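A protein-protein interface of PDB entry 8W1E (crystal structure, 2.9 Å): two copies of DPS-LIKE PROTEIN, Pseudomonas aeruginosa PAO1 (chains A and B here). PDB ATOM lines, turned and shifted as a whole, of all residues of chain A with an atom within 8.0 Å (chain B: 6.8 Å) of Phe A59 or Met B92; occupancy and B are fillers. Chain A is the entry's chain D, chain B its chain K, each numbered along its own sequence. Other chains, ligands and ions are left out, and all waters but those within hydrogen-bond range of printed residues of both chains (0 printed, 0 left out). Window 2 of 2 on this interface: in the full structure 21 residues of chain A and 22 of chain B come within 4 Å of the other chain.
NH1 of Arg A56 sits at hydrogen-bond distance from O of Pro B98, 2.8 Å away. NZ of Lys A55 is in salt-bridge range of OD1 of Asp B85 (2.6 Å). The backbone carbonyl oxygen (O) of Phe A59 lies close to the side-chain sulfur (SD) of Met B92 (3.4 Å). NH2 of Arg A56 is in salt-bridge range of OE1 of Glu B97 (2.9 Å).
Among the printed residues, pairs that only touch across the chains: Leu A52 with Phe B100 (3.5 Å), Lys A55 with Met B81 (3.3 Å), Lys A55 with Phe B100 (3.9 Å), Arg A56 with Phe B100 (3.8 Å), Phe A59 with Asp B85 (3.8 Å), Phe A59 with Ala B88 (3.5 Å), Phe A59 with Glu B89 (3.6 Å), Phe A59 with Pro B98 (3.9 Å), Phe A59 with Phe B100 (3.7 Å), Met A60 with Met B92 (3.8 Å), Met A60 with Glu B97 (3.6 Å) and Met A60 with Pro B98 (3.9 Å).
Phe A59 touches six residues of chain B. Of the printed residues of chain A, Ala B88 touches Phe A59. Printed residues of chain A within 4 Å of Glu B97: Arg A56 (2.9 Å) and Met A60 (3.6 Å). Of the printed residues of chain A, Phe B100 touches Leu A52 (3.5 Å), Lys A55 (3.9 Å), Arg A56 (3.8 Å) and Phe A59 (3.7 Å). The nearest residue of chain B that does not touch Phe A59 is Ala B84 (5.1 Å).
Of the 19 printed residues of chain B, 8 touch a printed residue of chain A. Hydrophobic or aromatic side chains of chain B that line the printed part of chain A: Met B81, Ala B88, Met B92, Pro B98 and Phe B100. Of the 16 printed residues of chain A, 5 touch a printed residue of chain B. Hydrophobic or aromatic side chains of chain A that line the printed part of chain B: Leu A52, Phe A59 and Met A60. Among the printed residues, 16 pairs touch across the chains.
No position is printed for both chains. Of the 16 pairs that touch across the chains among the printed residues, none has its exchanged pair printed and touching as well.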
ATOM      1  N   LEU A  52     -27.352 -30.328  32.021  1.00  0.00           N
ATOM      2  CA  LEU A  52     -28.066 -29.385  31.169  1.00  0.00           C
ATOM      3  C   LEU A  52     -28.123 -28.006  31.814  1.00  0.00           C
ATOM      4  O   LEU A  52     -27.961 -26.991  31.128  1.00  0.00           O
ATOM      5  CB  LEU A  52     -29.469 -29.910  30.876  1.00  0.00           C
ATOM      6  CG  LEU A  52     -29.523 -31.227  30.086  1.00  0.00           C
ATOM      7  CD1 LEU A  52     -30.951 -31.774  30.104  1.00  0.00           C
ATOM      8  CD2 LEU A  52     -29.034 -31.075  28.677  1.00  0.00           C
ATOM      9  N   ARG A  53     -28.355 -27.945  33.131  1.00  0.00           N
ATOM     10  CA  ARG A  53     -28.413 -26.649  33.804  1.00  0.00           C
ATOM     11  C   ARG A  53     -27.079 -25.918  33.697  1.00  0.00           C
ATOM     12  O   ARG A  53     -27.026 -24.739  33.327  1.00  0.00           O
ATOM     13  CB  ARG A  53     -28.799 -26.804  35.279  1.00  0.00           C
ATOM     14  CG  ARG A  53     -29.213 -25.462  35.940  1.00  0.00           C
ATOM     15  CD  ARG A  53     -29.043 -25.445  37.466  1.00  0.00           C
ATOM     16  NE  ARG A  53     -29.278 -26.765  38.027  1.00  0.00           N
ATOM     17  CZ  ARG A  53     -28.338 -27.532  38.556  1.00  0.00           C
ATOM     18  NH1 ARG A  53     -27.097 -27.098  38.710  1.00  0.00           N
ATOM     19  NH2 ARG A  53     -28.647 -28.775  38.919  1.00  0.00           N
ATOM     20  N   TYR A  54     -25.983 -26.609  34.016  1.00  0.00           N
ATOM     21  CA  TYR A  54     -24.672 -25.965  33.987  1.00  0.00           C
ATOM     22  C   TYR A  54     -24.323 -25.507  32.581  1.00  0.00           C
ATOM     23  O   TYR A  54     -23.772 -24.422  32.384  1.00  0.00           O
ATOM     24  CB  TYR A  54     -23.601 -26.921  34.505  1.00  0.00           C
ATOM     25  CG  TYR A  54     -23.321 -26.862  35.989  1.00  0.00           C
ATOM     26  CD1 TYR A  54     -22.886 -25.693  36.590  1.00  0.00           C
ATOM     27  CD2 TYR A  54     -23.446 -27.994  36.781  1.00  0.00           C
ATOM     28  CE1 TYR A  54     -22.601 -25.651  37.934  1.00  0.00           C
ATOM     29  CE2 TYR A  54     -23.157 -27.960  38.123  1.00  0.00           C
ATOM     30  CZ  TYR A  54     -22.732 -26.787  38.692  1.00  0.00           C
ATOM     31  OH  TYR A  54     -22.442 -26.746  40.031  1.00  0.00           O
ATOM     32  N   LYS A  55     -24.636 -26.327  31.590  1.00  0.00           N
ATOM     33  CA  LYS A  55     -24.356 -25.965  30.210  1.00  0.00           C
ATOM     34  C   LYS A  55     -25.102 -24.697  29.819  1.00  0.00           C
ATOM     35  O   LYS A  55     -24.534 -23.803  29.182  1.00  0.00           O
ATOM     36  CB  LYS A  55     -24.744 -27.141  29.327  1.00  0.00           C
ATOM     37  CG  LYS A  55     -23.829 -27.410  28.188  1.00  0.00           C
ATOM     38  CD  LYS A  55     -22.561 -28.113  28.595  1.00  0.00           C
ATOM     39  CE  LYS A  55     -21.565 -27.951  27.460  1.00  0.00           C
ATOM     40  NZ  LYS A  55     -22.070 -28.776  26.314  1.00  0.00           N
ATOM     41  N   ARG A  56     -26.372 -24.597  30.207  1.00  0.00           N
ATOM     42  CA  ARG A  56     -27.128 -23.366  29.986  1.00  0.00           C
ATOM     43  C   ARG A  56     -26.430 -22.179  30.641  1.00  0.00           C
ATOM     44  O   ARG A  56     -26.225 -21.135  30.007  1.00  0.00           O
ATOM     45  CB  ARG A  56     -28.555 -23.541  30.527  1.00  0.00           C
ATOM     46  CG  ARG A  56     -29.335 -22.269  30.797  1.00  0.00           C
ATOM     47  CD  ARG A  56     -29.815 -21.598  29.533  1.00  0.00           C
ATOM     48  NE  ARG A  56     -30.539 -20.370  29.820  1.00  0.00           N
ATOM     49  CZ  ARG A  56     -31.472 -19.860  29.029  1.00  0.00           C
ATOM     50  NH1 ARG A  56     -31.847 -20.478  27.919  1.00  0.00           N
ATOM     51  NH2 ARG A  56     -32.046 -18.704  29.360  1.00  0.00           N
ATOM     52  N   HIS A  57     -26.051 -22.324  31.915  1.00  0.00           N
ATOM     53  CA  HIS A  57     -25.393 -21.225  32.614  1.00  0.00           C
ATOM     54  C   HIS A  57     -24.057 -20.861  31.969  1.00  0.00           C
ATOM     55  O   HIS A  57     -23.680 -19.680  31.925  1.00  0.00           O
ATOM     56  CB  HIS A  57     -25.195 -21.579  34.087  1.00  0.00           C
ATOM     57  CG  HIS A  57     -26.471 -21.747  34.840  1.00  0.00           C
ATOM     58  ND1 HIS A  57     -26.509 -22.171  36.149  1.00  0.00           N
ATOM     59  CD2 HIS A  57     -27.758 -21.544  34.468  1.00  0.00           C
ATOM     60  CE1 HIS A  57     -27.765 -22.219  36.555  1.00  0.00           C
ATOM     61  NE2 HIS A  57     -28.543 -21.843  35.555  1.00  0.00           N
ATOM     62  N   TYR A  58     -23.317 -21.862  31.484  1.00  0.00           N
ATOM     63  CA  TYR A  58     -22.040 -21.582  30.838  1.00  0.00           C
ATOM     64  C   TYR A  58     -22.232 -20.638  29.666  1.00  0.00           C
ATOM     65  O   TYR A  58     -21.557 -19.608  29.565  1.00  0.00           O
ATOM     66  CB  TYR A  58     -21.384 -22.883  30.378  1.00  0.00           C
ATOM     67  CG  TYR A  58     -20.321 -22.687  29.324  1.00  0.00           C
ATOM     68  CD1 TYR A  58     -19.122 -22.075  29.628  1.00  0.00           C
ATOM     69  CD2 TYR A  58     -20.523 -23.111  28.032  1.00  0.00           C
ATOM     70  CE1 TYR A  58     -18.161 -21.884  28.674  1.00  0.00           C
ATOM     71  CE2 TYR A  58     -19.573 -22.934  27.074  1.00  0.00           C
ATOM     72  CZ  TYR A  58     -18.388 -22.318  27.392  1.00  0.00           C
ATOM     73  OH  TYR A  58     -17.417 -22.125  26.426  1.00  0.00           O
ATOM     74  N   PHE A  59     -23.186 -20.958  28.788  1.00  0.00           N
ATOM     75  CA  PHE A  59     -23.374 -20.164  27.581  1.00  0.00           C
ATOM     76  C   PHE A  59     -23.928 -18.781  27.891  1.00  0.00           C
ATOM     77  O   PHE A  59     -23.642 -17.830  27.153  1.00  0.00           O
ATOM     78  CB  PHE A  59     -24.305 -20.885  26.593  1.00  0.00           C
ATOM     79  CG  PHE A  59     -23.638 -21.997  25.824  1.00  0.00           C
ATOM     80  CD1 PHE A  59     -22.786 -21.712  24.774  1.00  0.00           C
ATOM     81  CD2 PHE A  59     -23.859 -23.317  26.155  1.00  0.00           C
ATOM     82  CE1 PHE A  59     -22.165 -22.713  24.080  1.00  0.00           C
ATOM     83  CE2 PHE A  59     -23.242 -24.322  25.456  1.00  0.00           C
ATOM     84  CZ  PHE A  59     -22.390 -24.017  24.415  1.00  0.00           C
ATOM     85  N   MET A  60     -24.732 -18.649  28.955  1.00  0.00           N
ATOM     86  CA  MET A  60     -25.387 -17.380  29.242  1.00  0.00           C
ATOM     87  C   MET A  60     -24.550 -16.431  30.083  1.00  0.00           C
ATOM     88  O   MET A  60     -24.823 -15.226  30.084  1.00  0.00           O
ATOM     89  CB  MET A  60     -26.717 -17.610  29.961  1.00  0.00           C
ATOM     90  CG  MET A  60     -27.767 -18.267  29.093  1.00  0.00           C
ATOM     91  SD  MET A  60     -28.388 -17.145  27.818  1.00  0.00           S
ATOM     92  CE  MET A  60     -29.213 -15.949  28.830  1.00  0.00           C
ATOM     93  N   ALA A  61     -23.525 -16.927  30.768  1.00  0.00           N
ATOM     94  CA  ALA A  61     -22.757 -16.084  31.679  1.00  0.00           C
ATOM     95  C   ALA A  61     -21.644 -15.388  30.899  1.00  0.00           C
ATOM     96  O   ALA A  61     -20.487 -15.819  30.862  1.00  0.00           O
ATOM     97  CB  ALA A  61     -22.198 -16.910  32.829  1.00  0.00           C
ATOM     98  N   THR A  62     -22.003 -14.264  30.288  1.00  0.00           N
ATOM     99  CA  THR A  62     -21.057 -13.455  29.538  1.00  0.00           C
ATOM    100  C   THR A  62     -20.713 -12.194  30.328  1.00  0.00           C
ATOM    101  O   THR A  62     -21.526 -11.670  31.106  1.00  0.00           O
ATOM    102  CB  THR A  62     -21.606 -13.057  28.163  1.00  0.00           C
ATOM    103  OG1 THR A  62     -22.505 -11.947  28.306  1.00  0.00           O
ATOM    104  CG2 THR A  62     -22.345 -14.209  27.545  1.00  0.00           C
ATOM    105  N   GLY A  63     -19.510 -11.694  30.075  1.00  0.00           N
ATOM    106  CA  GLY A  63     -18.930 -10.575  30.776  1.00  0.00           C
ATOM    107  C   GLY A  63     -17.557 -10.929  31.299  1.00  0.00           C
ATOM    108  O   GLY A  63     -17.077 -12.049  31.162  1.00  0.00           O
ATOM    109  N   ALA A  70     -18.410 -18.794  34.259  1.00  0.00           N
ATOM    110  CA  ALA A  70     -18.731 -19.643  33.116  1.00  0.00           C
ATOM    111  C   ALA A  70     -17.719 -20.771  32.980  1.00  0.00           C
ATOM    112  O   ALA A  70     -18.073 -21.902  32.623  1.00  0.00           O
ATOM    113  CB  ALA A  70     -18.785 -18.806  31.836  1.00  0.00           C
ATOM    114  N   PHE A  73     -18.639 -23.236  35.516  1.00  0.00           N
ATOM    115  CA  PHE A  73     -19.880 -23.881  35.095  1.00  0.00           C
ATOM    116  C   PHE A  73     -19.591 -25.002  34.105  1.00  0.00           C
ATOM    117  O   PHE A  73     -20.153 -26.097  34.195  1.00  0.00           O
ATOM    118  CB  PHE A  73     -20.837 -22.871  34.454  1.00  0.00           C
ATOM    119  CG  PHE A  73     -21.351 -21.820  35.390  1.00  0.00           C
ATOM    120  CD1 PHE A  73     -21.336 -22.010  36.762  1.00  0.00           C
ATOM    121  CD2 PHE A  73     -21.851 -20.632  34.890  1.00  0.00           C
ATOM    122  CE1 PHE A  73     -21.811 -21.036  37.616  1.00  0.00           C
ATOM    123  CE2 PHE A  73     -22.326 -19.665  35.737  1.00  0.00           C
ATOM    124  CZ  PHE A  73     -22.306 -19.867  37.104  1.00  0.00           C
ATOM    125  N   LEU A  74     -18.698 -24.747  33.157  1.00  0.00           N
ATOM    126  CA  LEU A  74     -18.425 -25.749  32.144  1.00  0.00           C
ATOM    127  C   LEU A  74     -17.695 -26.941  32.747  1.00  0.00           C
ATOM    128  O   LEU A  74     -18.030 -28.094  32.455  1.00  0.00           O
ATOM    129  CB  LEU A  74     -17.611 -25.123  31.023  1.00  0.00           C
ATOM    130  CG  LEU A  74     -17.358 -26.041  29.834  1.00  0.00           C
ATOM    131  CD1 LEU A  74     -18.635 -26.607  29.233  1.00  0.00           C
ATOM    132  CD2 LEU A  74     -16.610 -25.247  28.793  1.00  0.00           C
ATOM    133  N   MET A 122     -27.928 -17.855  38.775  1.00  0.00           N
ATOM    134  CA  MET A 122     -27.325 -19.078  38.253  1.00  0.00           C
ATOM    135  C   MET A 122     -26.498 -19.755  39.335  1.00  0.00           C
ATOM    136  O   MET A 122     -26.682 -20.944  39.625  1.00  0.00           O
ATOM    137  CB  MET A 122     -26.475 -18.758  37.015  1.00  0.00           C
ATOM    138  CG  MET A 122     -27.327 -18.317  35.825  1.00  0.00           C
ATOM    139  SD  MET A 122     -26.463 -17.830  34.318  1.00  0.00           S
ATOM    140  CE  MET A 122     -25.262 -16.677  34.904  1.00  0.00           C
ATOM    141  N   LEU B  37     -32.625 -17.855  14.845  1.00  0.00           N
ATOM    142  CA  LEU B  37     -32.499 -18.298  16.227  1.00  0.00           C
ATOM    143  C   LEU B  37     -33.490 -19.410  16.538  1.00  0.00           C
ATOM    144  O   LEU B  37     -33.176 -20.343  17.289  1.00  0.00           O
ATOM    145  CB  LEU B  37     -32.724 -17.136  17.191  1.00  0.00           C
ATOM    146  CG  LEU B  37     -31.579 -16.147  17.363  1.00  0.00           C
ATOM    147  CD1 LEU B  37     -32.016 -14.967  18.209  1.00  0.00           C
ATOM    148  CD2 LEU B  37     -30.360 -16.834  17.955  1.00  0.00           C
ATOM    149  N   LEU B  40     -32.034 -22.512  15.019  1.00  0.00           N
ATOM    150  CA  LEU B  40     -30.876 -22.930  15.794  1.00  0.00           C
ATOM    151  C   LEU B  40     -31.304 -23.675  17.051  1.00  0.00           C
ATOM    152  O   LEU B  40     -30.689 -24.682  17.422  1.00  0.00           O
ATOM    153  CB  LEU B  40     -30.026 -21.717  16.166  1.00  0.00           C
ATOM    154  CG  LEU B  40     -29.198 -21.154  15.011  1.00  0.00           C
ATOM    155  CD1 LEU B  40     -28.591 -19.802  15.338  1.00  0.00           C
ATOM    156  CD2 LEU B  40     -28.129 -22.172  14.643  1.00  0.00           C
ATOM    157  N   MET B  81     -23.163 -34.014  20.571  1.00  0.00           N
ATOM    158  CA  MET B  81     -22.954 -32.994  21.582  1.00  0.00           C
ATOM    159  C   MET B  81     -22.062 -31.877  21.053  1.00  0.00           C
ATOM    160  O   MET B  81     -22.264 -30.708  21.401  1.00  0.00           O
ATOM    161  CB  MET B  81     -22.354 -33.616  22.835  1.00  0.00           C
ATOM    162  CG  MET B  81     -22.471 -32.720  24.052  1.00  0.00           C
ATOM    163  SD  MET B  81     -24.130 -32.709  24.696  1.00  0.00           S
ATOM    164  CE  MET B  81     -24.299 -30.946  25.071  1.00  0.00           C
ATOM    165  N   ALA B  84     -24.357 -29.774  19.284  1.00  0.00           N
ATOM    166  CA  ALA B  84     -25.107 -28.999  20.264  1.00  0.00           C
ATOM    167  C   ALA B  84     -24.326 -27.762  20.693  1.00  0.00           C
ATOM    168  O   ALA B  84     -24.878 -26.662  20.789  1.00  0.00           O
ATOM    169  CB  ALA B  84     -25.429 -29.877  21.473  1.00  0.00           C
ATOM    170  N   ASP B  85     -23.035 -27.934  20.973  1.00  0.00           N
ATOM    171  CA  ASP B  85     -22.202 -26.812  21.393  1.00  0.00           C
ATOM    172  C   ASP B  85     -22.035 -25.788  20.274  1.00  0.00           C
ATOM    173  O   ASP B  85     -22.120 -24.579  20.521  1.00  0.00           O
ATOM    174  CB  ASP B  85     -20.851 -27.341  21.884  1.00  0.00           C
ATOM    175  CG  ASP B  85     -20.907 -27.876  23.318  1.00  0.00           C
ATOM    176  OD1 ASP B  85     -21.995 -27.793  23.957  1.00  0.00           O
ATOM    177  OD2 ASP B  85     -19.858 -28.377  23.794  1.00  0.00           O
ATOM    178  N   GLN B  86     -21.796 -26.246  19.044  1.00  0.00           N
ATOM    179  CA  GLN B  86     -21.677 -25.317  17.925  1.00  0.00           C
ATOM    180  C   GLN B  86     -22.928 -24.455  17.817  1.00  0.00           C
ATOM    181  O   GLN B  86     -22.854 -23.232  17.655  1.00  0.00           O
ATOM    182  CB  GLN B  86     -21.489 -26.094  16.625  1.00  0.00           C
ATOM    183  CG  GLN B  86     -20.080 -26.440  16.210  1.00  0.00           C
ATOM    184  CD  GLN B  86     -20.058 -27.176  14.856  1.00  0.00           C
ATOM    185  OE1 GLN B  86     -19.800 -28.401  14.784  1.00  0.00           O
ATOM    186  NE2 GLN B  86     -20.350 -26.436  13.781  1.00  0.00           N
ATOM    187  N   LEU B  87     -24.094 -25.097  17.899  1.00  0.00           N
ATOM    188  CA  LEU B  87     -25.358 -24.399  17.733  1.00  0.00           C
ATOM    189  C   LEU B  87     -25.606 -23.436  18.882  1.00  0.00           C
ATOM    190  O   LEU B  87     -26.008 -22.290  18.659  1.00  0.00           O
ATOM    191  CB  LEU B  87     -26.486 -25.429  17.611  1.00  0.00           C
ATOM    192  CG  LEU B  87     -26.410 -26.354  16.393  1.00  0.00           C
ATOM    193  CD1 LEU B  87     -27.199 -27.634  16.635  1.00  0.00           C
ATOM    194  CD2 LEU B  87     -26.943 -25.674  15.126  1.00  0.00           C
ATOM    195  N   ALA B  88     -25.357 -23.872  20.115  1.00  0.00           N
ATOM    196  CA  ALA B  88     -25.553 -22.988  21.258  1.00  0.00           C
ATOM    197  C   ALA B  88     -24.637 -21.769  21.174  1.00  0.00           C
ATOM    198  O   ALA B  88     -25.069 -20.640  21.433  1.00  0.00           O
ATOM    199  CB  ALA B  88     -25.318 -23.767  22.553  1.00  0.00           C
ATOM    200  N   GLU B  89     -23.372 -21.980  20.803  1.00  0.00           N
ATOM    201  CA  GLU B  89     -22.443 -20.872  20.608  1.00  0.00           C
ATOM    202  C   GLU B  89     -22.992 -19.846  19.622  1.00  0.00           C
ATOM    203  O   GLU B  89     -22.850 -18.634  19.825  1.00  0.00           O
ATOM    204  CB  GLU B  89     -21.104 -21.423  20.101  1.00  0.00           C
ATOM    205  CG  GLU B  89     -20.039 -20.369  19.821  1.00  0.00           C
ATOM    206  CD  GLU B  89     -18.737 -20.956  19.283  1.00  0.00           C
ATOM    207  OE1 GLU B  89     -18.611 -22.205  19.239  1.00  0.00           O
ATOM    208  OE2 GLU B  89     -17.847 -20.158  18.898  1.00  0.00           O
ATOM    209  N   ARG B  90     -23.614 -20.315  18.540  1.00  0.00           N
ATOM    210  CA  ARG B  90     -24.122 -19.401  17.524  1.00  0.00           C
ATOM    211  C   ARG B  90     -25.360 -18.672  18.021  1.00  0.00           C
ATOM    212  O   ARG B  90     -25.554 -17.489  17.725  1.00  0.00           O
ATOM    213  CB  ARG B  90     -24.430 -20.179  16.245  1.00  0.00           C
ATOM    214  CG  ARG B  90     -24.793 -19.322  15.051  1.00  0.00           C
ATOM    215  CD  ARG B  90     -23.697 -18.321  14.750  1.00  0.00           C
ATOM    216  NE  ARG B  90     -24.003 -17.536  13.564  1.00  0.00           N
ATOM    217  CZ  ARG B  90     -23.422 -16.387  13.264  1.00  0.00           C
ATOM    218  NH1 ARG B  90     -22.509 -15.854  14.059  1.00  0.00           N
ATOM    219  NH2 ARG B  90     -23.772 -15.750  12.148  1.00  0.00           N
ATOM    220  N   ILE B  91     -26.222 -19.374  18.757  1.00  0.00           N
ATOM    221  CA  ILE B  91     -27.378 -18.733  19.370  1.00  0.00           C
ATOM    222  C   ILE B  91     -26.920 -17.539  20.192  1.00  0.00           C
ATOM    223  O   ILE B  91     -27.524 -16.458  20.149  1.00  0.00           O
ATOM    224  CB  ILE B  91     -28.168 -19.752  20.219  1.00  0.00           C
ATOM    225  CG1 ILE B  91     -28.894 -20.736  19.292  1.00  0.00           C
ATOM    226  CG2 ILE B  91     -29.137 -19.038  21.176  1.00  0.00           C
ATOM    227  CD1 ILE B  91     -29.513 -21.914  19.992  1.00  0.00           C
ATOM    228  N   MET B  92     -25.829 -17.700  20.937  1.00  0.00           N
ATOM    229  CA  MET B  92     -25.376 -16.581  21.751  1.00  0.00           C
ATOM    230  C   MET B  92     -24.899 -15.425  20.879  1.00  0.00           C
ATOM    231  O   MET B  92     -25.258 -14.272  21.123  1.00  0.00           O
ATOM    232  CB  MET B  92     -24.275 -17.032  22.704  1.00  0.00           C
ATOM    233  CG  MET B  92     -24.712 -18.055  23.738  1.00  0.00           C
ATOM    234  SD  MET B  92     -26.073 -17.464  24.765  1.00  0.00           S
ATOM    235  CE  MET B  92     -25.413 -15.965  25.444  1.00  0.00           C
ATOM    236  N   GLN B  93     -24.147 -15.721  19.816  1.00  0.00           N
ATOM    237  CA  GLN B  93     -23.606 -14.661  18.973  1.00  0.00           C
ATOM    238  C   GLN B  93     -24.701 -13.832  18.316  1.00  0.00           C
ATOM    239  O   GLN B  93     -24.525 -12.620  18.121  1.00  0.00           O
ATOM    240  CB  GLN B  93     -22.702 -15.269  17.907  1.00  0.00           C
ATOM    241  CG  GLN B  93     -21.393 -15.765  18.443  1.00  0.00           C
ATOM    242  CD  GLN B  93     -20.674 -16.659  17.469  1.00  0.00           C
ATOM    243  OE1 GLN B  93     -21.224 -17.039  16.440  1.00  0.00           O
ATOM    244  NE2 GLN B  93     -19.434 -17.001  17.791  1.00  0.00           N
ATOM    245  N   LEU B  94     -25.827 -14.457  17.977  1.00  0.00           N
ATOM    246  CA  LEU B  94     -26.958 -13.788  17.350  1.00  0.00           C
ATOM    247  C   LEU B  94     -27.932 -13.233  18.374  1.00  0.00           C
ATOM    248  O   LEU B  94     -29.064 -12.895  18.014  1.00  0.00           O
ATOM    249  CB  LEU B  94     -27.688 -14.753  16.411  1.00  0.00           C
ATOM    250  CG  LEU B  94     -26.857 -15.258  15.233  1.00  0.00           C
ATOM    251  CD1 LEU B  94     -27.577 -16.265  14.365  1.00  0.00           C
ATOM    252  CD2 LEU B  94     -26.443 -14.068  14.366  1.00  0.00           C
ATOM    253  N   GLY B  95     -27.545 -13.213  19.647  1.00  0.00           N
ATOM    254  CA  GLY B  95     -28.317 -12.532  20.664  1.00  0.00           C
ATOM    255  C   GLY B  95     -29.517 -13.275  21.198  1.00  0.00           C
ATOM    256  O   GLY B  95     -30.438 -12.641  21.723  1.00  0.00           O
ATOM    257  N   GLY B  96     -29.512 -14.606  21.132  1.00  0.00           N
ATOM    258  CA  GLY B  96     -30.587 -15.416  21.645  1.00  0.00           C
ATOM    259  C   GLY B  96     -30.197 -16.105  22.941  1.00  0.00           C
ATOM    260  O   GLY B  96     -29.194 -15.775  23.579  1.00  0.00           O
ATOM    261  N   GLU B  97     -31.026 -17.067  23.339  1.00  0.00           N
ATOM    262  CA  GLU B  97     -30.768 -17.864  24.536  1.00  0.00           C
ATOM    263  C   GLU B  97     -30.893 -19.323  24.124  1.00  0.00           C
ATOM    264  O   GLU B  97     -31.954 -19.726  23.609  1.00  0.00           O
ATOM    265  CB  GLU B  97     -31.741 -17.524  25.676  1.00  0.00           C
ATOM    266  CG  GLU B  97     -31.684 -16.063  26.175  1.00  0.00           C
ATOM    267  CD  GLU B  97     -32.618 -15.759  27.364  1.00  0.00           C
ATOM    268  OE1 GLU B  97     -33.394 -16.651  27.775  1.00  0.00           O
ATOM    269  OE2 GLU B  97     -32.578 -14.615  27.884  1.00  0.00           O
ATOM    270  N   PRO B  98     -29.881 -20.161  24.355  1.00  0.00           N
ATOM    271  CA  PRO B  98     -29.998 -21.579  23.979  1.00  0.00           C
ATOM    272  C   PRO B  98     -30.792 -22.329  25.032  1.00  0.00           C
ATOM    273  O   PRO B  98     -30.510 -22.220  26.226  1.00  0.00           O
ATOM    274  CB  PRO B  98     -28.545 -22.062  23.939  1.00  0.00           C
ATOM    275  CG  PRO B  98     -27.873 -21.242  24.985  1.00  0.00           C
ATOM    276  CD  PRO B  98     -28.579 -19.875  24.989  1.00  0.00           C
ATOM    277  N   PHE B 100     -31.634 -25.404  26.906  1.00  0.00           N
ATOM    278  CA  PHE B 100     -31.246 -26.733  27.363  1.00  0.00           C
ATOM    279  C   PHE B 100     -32.284 -27.379  28.280  1.00  0.00           C
ATOM    280  O   PHE B 100     -31.997 -28.416  28.889  1.00  0.00           O
ATOM    281  CB  PHE B 100     -29.902 -26.668  28.098  1.00  0.00           C
ATOM    282  CG  PHE B 100     -28.718 -26.457  27.197  1.00  0.00           C
ATOM    283  CD1 PHE B 100     -28.029 -27.536  26.685  1.00  0.00           C
ATOM    284  CD2 PHE B 100     -28.290 -25.182  26.870  1.00  0.00           C
ATOM    285  CE1 PHE B 100     -26.934 -27.355  25.863  1.00  0.00           C
ATOM    286  CE2 PHE B 100     -27.206 -25.001  26.041  1.00  0.00           C
ATOM    287  CZ  PHE B 100     -26.524 -26.088  25.542  1.00  0.00           C
